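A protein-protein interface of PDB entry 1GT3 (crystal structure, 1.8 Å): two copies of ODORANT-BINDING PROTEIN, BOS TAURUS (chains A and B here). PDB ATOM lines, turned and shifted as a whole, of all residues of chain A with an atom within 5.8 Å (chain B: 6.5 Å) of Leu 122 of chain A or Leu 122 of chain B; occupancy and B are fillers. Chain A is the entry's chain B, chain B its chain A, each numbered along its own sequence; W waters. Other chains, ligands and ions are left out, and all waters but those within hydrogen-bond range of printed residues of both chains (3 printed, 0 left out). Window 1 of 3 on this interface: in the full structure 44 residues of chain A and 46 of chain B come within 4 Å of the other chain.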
ATOM      1  N   PRO A  16      25.182 -19.500 -12.029  1.00  0.00           N
ATOM      2  CA  PRO A  16      24.479 -20.009 -13.208  1.00  0.00           C
ATOM      3  C   PRO A  16      22.994 -19.655 -13.235  1.00  0.00           C
ATOM      4  O   PRO A  16      22.274 -19.859 -12.255  1.00  0.00           O
ATOM      5  CB  PRO A  16      24.723 -21.511 -13.126  1.00  0.00           C
ATOM      6  CG  PRO A  16      24.736 -21.760 -11.654  1.00  0.00           C
ATOM      7  CD  PRO A  16      25.548 -20.595 -11.112  1.00  0.00           C
ATOM      8  N   TRP A  17      22.559 -19.102 -14.362  1.00  0.00           N
ATOM      9  CA  TRP A  17      21.162 -18.732 -14.571  1.00  0.00           C
ATOM     10  C   TRP A  17      20.733 -19.293 -15.916  1.00  0.00           C
ATOM     11  O   TRP A  17      21.561 -19.460 -16.818  1.00  0.00           O
ATOM     12  CB  TRP A  17      20.989 -17.212 -14.590  1.00  0.00           C
ATOM     13  CG  TRP A  17      21.012 -16.576 -13.234  1.00  0.00           C
ATOM     14  CD1 TRP A  17      22.111 -16.280 -12.488  1.00  0.00           C
ATOM     15  CD2 TRP A  17      19.875 -16.148 -12.470  1.00  0.00           C
ATOM     16  NE1 TRP A  17      21.735 -15.683 -11.304  1.00  0.00           N
ATOM     17  CE2 TRP A  17      20.369 -15.590 -11.267  1.00  0.00           C
ATOM     18  CE3 TRP A  17      18.488 -16.180 -12.687  1.00  0.00           C
ATOM     19  CZ2 TRP A  17      19.520 -15.065 -10.274  1.00  0.00           C
ATOM     20  CZ3 TRP A  17      17.638 -15.659 -11.697  1.00  0.00           C
ATOM     21  CH2 TRP A  17      18.164 -15.108 -10.506  1.00  0.00           C
ATOM     22  N   ARG A  18      19.443 -19.572 -16.058  1.00  0.00           N
ATOM     23  CA  ARG A  18      18.914 -20.120 -17.303  1.00  0.00           C
ATOM     24  C   ARG A  18      17.676 -19.373 -17.787  1.00  0.00           C
ATOM     25  O   ARG A  18      16.864 -18.909 -16.993  1.00  0.00           O
ATOM     26  CB  ARG A  18      18.565 -21.604 -17.117  1.00  0.00           C
ATOM     27  CG  ARG A  18      19.767 -22.502 -16.925  1.00  0.00           C
ATOM     28  CD  ARG A  18      20.757 -22.708 -18.052  1.00  0.00           C
ATOM     29  NE  ARG A  18      21.859 -23.591 -17.678  1.00  0.00           N
ATOM     30  CZ  ARG A  18      23.027 -23.184 -17.184  1.00  0.00           C
ATOM     31  NH1 ARG A  18      23.957 -24.078 -16.878  1.00  0.00           N
ATOM     32  NH2 ARG A  18      23.271 -21.892 -17.012  1.00  0.00           N
ATOM     33  N   VAL A 120      15.675 -18.302 -14.426  1.00  0.00           N
ATOM     34  CA  VAL A 120      15.738 -19.041 -13.176  1.00  0.00           C
ATOM     35  C   VAL A 120      17.192 -19.347 -12.835  1.00  0.00           C
ATOM     36  O   VAL A 120      18.027 -19.567 -13.721  1.00  0.00           O
ATOM     37  CB  VAL A 120      14.912 -20.367 -13.279  1.00  0.00           C
ATOM     38  CG1 VAL A 120      15.472 -21.252 -14.376  1.00  0.00           C
ATOM     39  CG2 VAL A 120      14.934 -21.114 -11.959  1.00  0.00           C
ATOM     40  N   LYS A 121      17.500 -19.345 -11.550  1.00  0.00           N
ATOM     41  CA  LYS A 121      18.856 -19.630 -11.125  1.00  0.00           C
ATOM     42  C   LYS A 121      19.029 -21.099 -10.770  1.00  0.00           C
ATOM     43  O   LYS A 121      18.120 -21.728 -10.235  1.00  0.00           O
ATOM     44  CB  LYS A 121      19.217 -18.776  -9.916  1.00  0.00           C
ATOM     45  CG  LYS A 121      20.642 -18.987  -9.462  1.00  0.00           C
ATOM     46  CD  LYS A 121      21.173 -18.327  -8.247  1.00  0.00           C
ATOM     47  CE  LYS A 121      22.612 -18.590  -7.854  1.00  0.00           C
ATOM     48  NZ  LYS A 121      22.935 -17.920  -6.578  1.00  0.00           N
ATOM     49  N   LEU A 122      20.194 -21.652 -11.091  1.00  0.00           N
ATOM     50  CA  LEU A 122      20.479 -23.037 -10.744  1.00  0.00           C
ATOM     51  C   LEU A 122      21.237 -22.974  -9.430  1.00  0.00           C
ATOM     52  O   LEU A 122      22.381 -22.524  -9.391  1.00  0.00           O
ATOM     53  CB  LEU A 122      21.350 -23.705 -11.806  1.00  0.00           C
ATOM     54  CG  LEU A 122      20.630 -24.405 -12.959  1.00  0.00           C
ATOM     55  CD1 LEU A 122      19.725 -23.423 -13.678  1.00  0.00           C
ATOM     56  CD2 LEU A 122      21.658 -24.999 -13.910  1.00  0.00           C
ATOM     57  N   ASN A 123      20.595 -23.416  -8.356  1.00  0.00           N
ATOM     58  CA  ASN A 123      21.213 -23.386  -7.038  1.00  0.00           C
ATOM     59  C   ASN A 123      21.749 -24.727  -6.565  1.00  0.00           C
ATOM     60  O   ASN A 123      21.028 -25.719  -6.527  1.00  0.00           O
ATOM     61  CB  ASN A 123      20.218 -22.866  -5.999  1.00  0.00           C
ATOM     62  CG  ASN A 123      20.288 -21.363  -5.825  1.00  0.00           C
ATOM     63  OD1 ASN A 123      21.328 -20.814  -5.458  1.00  0.00           O
ATOM     64  ND2 ASN A 123      19.177 -20.692  -6.086  1.00  0.00           N
ATOM     65  N   VAL A 124      23.027 -24.745  -6.208  1.00  0.00           N
ATOM     66  CA  VAL A 124      23.663 -25.949  -5.696  1.00  0.00           C
ATOM     67  C   VAL A 124      24.026 -25.664  -4.244  1.00  0.00           C
ATOM     68  O   VAL A 124      24.901 -24.845  -3.971  1.00  0.00           O
ATOM     69  CB  VAL A 124      24.942 -26.289  -6.481  1.00  0.00           C
ATOM     70  CG1 VAL A 124      25.627 -27.501  -5.861  1.00  0.00           C
ATOM     71  CG2 VAL A 124      24.594 -26.563  -7.932  1.00  0.00           C
ATOM     72  N   LEU A 150      28.072 -28.895 -15.067  1.00  0.00           N
ATOM     73  CA  LEU A 150      27.539 -27.543 -14.951  1.00  0.00           C
ATOM     74  C   LEU A 150      28.458 -26.488 -15.556  1.00  0.00           C
ATOM     75  O   LEU A 150      27.991 -25.571 -16.240  1.00  0.00           O
ATOM     76  CB  LEU A 150      27.245 -27.217 -13.481  1.00  0.00           C
ATOM     77  CG  LEU A 150      26.690 -25.820 -13.183  1.00  0.00           C
ATOM     78  CD1 LEU A 150      25.398 -25.600 -13.951  1.00  0.00           C
ATOM     79  CD2 LEU A 150      26.451 -25.676 -11.686  1.00  0.00           C
ATOM     80  N   GLU A 153      28.301 -26.660 -19.404  1.00  0.00           N
ATOM     81  CA  GLU A 153      27.145 -25.953 -19.938  1.00  0.00           C
ATOM     82  C   GLU A 153      27.291 -24.438 -19.799  1.00  0.00           C
ATOM     83  O   GLU A 153      26.775 -23.698 -20.627  1.00  0.00           O
ATOM     84  CB  GLU A 153      25.856 -26.399 -19.242  1.00  0.00           C
ATOM     85  CG  GLU A 153      25.405 -27.839 -19.580  1.00  0.00           C
ATOM     86  CD  GLU A 153      23.960 -28.091 -19.171  1.00  0.00           C
ATOM     87  OE1 GLU A 153      23.501 -29.246 -19.227  1.00  0.00           O
ATOM     88  OE2 GLU A 153      23.279 -27.120 -18.796  1.00  0.00           O
ATOM     89  N   GLY B  15       9.965 -32.855 -13.696  1.00  0.00           N
ATOM     90  CA  GLY B  15      10.250 -31.579 -14.317  1.00  0.00           C
ATOM     91  C   GLY B  15      11.642 -31.523 -14.905  1.00  0.00           C
ATOM     92  O   GLY B  15      12.293 -32.555 -15.073  1.00  0.00           O
ATOM     93  N   PRO B  16      12.118 -30.323 -15.254  1.00  0.00           N
ATOM     94  CA  PRO B  16      13.458 -30.189 -15.828  1.00  0.00           C
ATOM     95  C   PRO B  16      14.545 -30.342 -14.769  1.00  0.00           C
ATOM     96  O   PRO B  16      14.501 -29.713 -13.714  1.00  0.00           O
ATOM     97  CB  PRO B  16      13.426 -28.795 -16.462  1.00  0.00           C
ATOM     98  CG  PRO B  16      12.429 -28.050 -15.614  1.00  0.00           C
ATOM     99  CD  PRO B  16      11.350 -29.069 -15.376  1.00  0.00           C
ATOM    100  N   TRP B  17      15.515 -31.206 -15.059  1.00  0.00           N
ATOM    101  CA  TRP B  17      16.633 -31.458 -14.159  1.00  0.00           C
ATOM    102  C   TRP B  17      17.918 -31.317 -14.956  1.00  0.00           C
ATOM    103  O   TRP B  17      17.927 -31.506 -16.174  1.00  0.00           O
ATOM    104  CB  TRP B  17      16.572 -32.878 -13.571  1.00  0.00           C
ATOM    105  CG  TRP B  17      15.531 -33.084 -12.520  1.00  0.00           C
ATOM    106  CD1 TRP B  17      14.186 -33.228 -12.710  1.00  0.00           C
ATOM    107  CD2 TRP B  17      15.746 -33.160 -11.105  1.00  0.00           C
ATOM    108  NE1 TRP B  17      13.549 -33.385 -11.504  1.00  0.00           N
ATOM    109  CE2 TRP B  17      14.482 -33.349 -10.502  1.00  0.00           C
ATOM    110  CE3 TRP B  17      16.883 -33.086 -10.291  1.00  0.00           C
ATOM    111  CZ2 TRP B  17      14.322 -33.466  -9.119  1.00  0.00           C
ATOM    112  CZ3 TRP B  17      16.726 -33.198  -8.912  1.00  0.00           C
ATOM    113  CH2 TRP B  17      15.452 -33.388  -8.342  1.00  0.00           C
ATOM    114  N   ARG B  18      19.000 -30.989 -14.262  1.00  0.00           N
ATOM    115  CA  ARG B  18      20.297 -30.820 -14.903  1.00  0.00           C
ATOM    116  C   ARG B  18      21.394 -31.574 -14.168  1.00  0.00           C
ATOM    117  O   ARG B  18      21.352 -31.726 -12.957  1.00  0.00           O
ATOM    118  CB  ARG B  18      20.662 -29.329 -14.958  1.00  0.00           C
ATOM    119  CG  ARG B  18      19.784 -28.503 -15.922  1.00  0.00           C
ATOM    120  CD  ARG B  18      19.828 -28.804 -17.432  1.00  0.00           C
ATOM    121  NE  ARG B  18      18.952 -27.933 -18.218  1.00  0.00           N
ATOM    122  CZ  ARG B  18      17.668 -28.181 -18.479  1.00  0.00           C
ATOM    123  NH1 ARG B  18      17.082 -29.279 -18.018  1.00  0.00           N
ATOM    124  NH2 ARG B  18      16.972 -27.334 -19.223  1.00  0.00           N
ATOM    125  N   THR B  97      14.869 -29.914  -4.691  1.00  0.00           N
ATOM    126  CA  THR B  97      15.862 -29.285  -5.553  1.00  0.00           C
ATOM    127  C   THR B  97      17.072 -30.122  -5.954  1.00  0.00           C
ATOM    128  O   THR B  97      17.778 -29.760  -6.894  1.00  0.00           O
ATOM    129  CB  THR B  97      16.388 -27.987  -4.921  1.00  0.00           C
ATOM    130  OG1 THR B  97      17.089 -28.300  -3.714  1.00  0.00           O
ATOM    131  CG2 THR B  97      15.239 -27.049  -4.596  1.00  0.00           C
ATOM    132  N   VAL B 120      20.414 -31.317 -10.232  1.00  0.00           N
ATOM    133  CA  VAL B 120      19.636 -30.256  -9.614  1.00  0.00           C
ATOM    134  C   VAL B 120      18.416 -29.953 -10.451  1.00  0.00           C
ATOM    135  O   VAL B 120      18.444 -30.045 -11.680  1.00  0.00           O
ATOM    136  CB  VAL B 120      20.467 -28.965  -9.433  1.00  0.00           C
ATOM    137  CG1 VAL B 120      21.612 -29.231  -8.480  1.00  0.00           C
ATOM    138  CG2 VAL B 120      20.985 -28.471 -10.775  1.00  0.00           C
ATOM    139  N   LYS B 121      17.331 -29.597  -9.782  1.00  0.00           N
ATOM    140  CA  LYS B 121      16.103 -29.312 -10.488  1.00  0.00           C
ATOM    141  C   LYS B 121      15.914 -27.831 -10.772  1.00  0.00           C
ATOM    142  O   LYS B 121      16.251 -26.981  -9.947  1.00  0.00           O
ATOM    143  CB  LYS B 121      14.918 -29.838  -9.692  1.00  0.00           C
ATOM    144  CG  LYS B 121      13.619 -29.668 -10.391  1.00  0.00           C
ATOM    145  CD  LYS B 121      12.348 -30.064  -9.727  1.00  0.00           C
ATOM    146  CE  LYS B 121      11.054 -29.861 -10.491  1.00  0.00           C
ATOM    147  NZ  LYS B 121       9.888 -30.313  -9.706  1.00  0.00           N
ATOM    148  N   LEU B 122      15.398 -27.535 -11.956  1.00  0.00           N
ATOM    149  CA  LEU B 122      15.125 -26.161 -12.353  1.00  0.00           C
ATOM    150  C   LEU B 122      13.671 -25.906 -11.996  1.00  0.00           C
ATOM    151  O   LEU B 122      12.765 -26.273 -12.735  1.00  0.00           O
ATOM    152  CB  LEU B 122      15.345 -25.972 -13.853  1.00  0.00           C
ATOM    153  CG  LEU B 122      16.810 -25.882 -14.292  1.00  0.00           C
ATOM    154  CD1 LEU B 122      17.562 -27.135 -13.875  1.00  0.00           C
ATOM    155  CD2 LEU B 122      16.875 -25.701 -15.790  1.00  0.00           C
ATOM    156  N   ASN B 123      13.462 -25.293 -10.841  1.00  0.00           N
ATOM    157  CA  ASN B 123      12.119 -25.011 -10.363  1.00  0.00           C
ATOM    158  C   ASN B 123      11.570 -23.679 -10.854  1.00  0.00           C
ATOM    159  O   ASN B 123      12.218 -22.647 -10.719  1.00  0.00           O
ATOM    160  CB  ASN B 123      12.105 -25.043  -8.835  1.00  0.00           C
ATOM    161  CG  ASN B 123      12.342 -26.435  -8.287  1.00  0.00           C
ATOM    162  OD1 ASN B 123      11.579 -27.355  -8.577  1.00  0.00           O
ATOM    163  ND2 ASN B 123      13.401 -26.597  -7.499  1.00  0.00           N
ATOM    164  N   VAL B 124      10.380 -23.717 -11.440  1.00  0.00           N
ATOM    165  CA  VAL B 124       9.729 -22.505 -11.927  1.00  0.00           C
ATOM    166  C   VAL B 124       8.443 -22.348 -11.122  1.00  0.00           C
ATOM    167  O   VAL B 124       7.497 -23.124 -11.279  1.00  0.00           O
ATOM    168  CB  VAL B 124       9.401 -22.595 -13.438  1.00  0.00           C
ATOM    169  CG1 VAL B 124       8.749 -21.298 -13.908  1.00  0.00           C
ATOM    170  CG2 VAL B 124      10.676 -22.852 -14.231  1.00  0.00           C
ATOM    171  N   LEU B 150      13.091 -23.772 -22.247  1.00  0.00           N
ATOM    172  CA  LEU B 150      13.311 -24.948 -21.409  1.00  0.00           C
ATOM    173  C   LEU B 150      13.097 -26.235 -22.192  1.00  0.00           C
ATOM    174  O   LEU B 150      13.819 -27.214 -22.002  1.00  0.00           O
ATOM    175  CB  LEU B 150      12.388 -24.900 -20.189  1.00  0.00           C
ATOM    176  CG  LEU B 150      13.075 -24.916 -18.818  1.00  0.00           C
ATOM    177  CD1 LEU B 150      14.252 -23.950 -18.792  1.00  0.00           C
ATOM    178  CD2 LEU B 150      12.059 -24.557 -17.748  1.00  0.00           C
HETATM  179  O   HOH W   1      21.004 -26.205 -19.127  1.00  0.00           O
HETATM  180  O   HOH W   2      15.904 -23.381 -10.123  1.00  0.00           O
HETATM  181  O   HOH W   3      17.803 -24.985  -8.710  1.00  0.00           O
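The backbone carbonyl oxygen (O) of Pro 16 of chain B lies within hydrogen-bond range of the backbone NH (N) of Leu 122 of chain B.
O of Pro 16 of chain A lies within hydrogen-bond range of N of Leu 122 of chain A (3.0 Å).
N of Arg 18 of chain A sits at hydrogen-bond distance from O of Val 120 of chain A (2.7 Å).
Val 120 of chain A touches Asn 123 of chain B (CG2 to O, 3.4 Å).
CG of Leu 122 of chain B touches CD1 of Leu 122 of chain A, 3.9 Å away.
Of the printed residues of chain B, Val 120 of chain A touches Asn 123.
Lys 121 of chain A touches none of the printed residues of chain B.
Leu 122 of chain A touches one residue of chain B.
Printed residues of chain A within 4 Å of Asn 123 of chain B: Val 120.
Hydrophobic or aromatic side chains of chain B that line the printed part of chain A: Leu 122.
Of the 10 printed residues of chain A, 2 touch a printed residue of chain B.
Val 120 of chain A touches Asn 123 of chain B, but with the chains exchanged Asn 123 of chain A does not touch Val 120 of chain B (4.1 Å).
Leu 122 of chain B touches its own counterpart, Leu 122 of chain A.
Positions printed for both chains: 16, 17, 18, 120, 121, 122, 123, 124 and 150.
Of the 2 pairs that touch across the chains among the printed residues, 1 has its exchanged pair printed and touching as well.
Water W1 lies within hydrogen-bond range of the side-chain carboxylate (OE2) of Glu 153 of chain A (2.5 Å), the guanidinium group (NE) of Arg 18 of chain B (2.8 Å) and the guanidinium group (NE) of Arg 18 of chain A (3.1 Å).
Water W2 bridges O of Lys 121 of chain A (2.8 Å) and N of Asn 123 of chain B (3.2 Å).
Water W3 bridges O of Lys 121 of chain B and N of Asn 123 of chain A.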
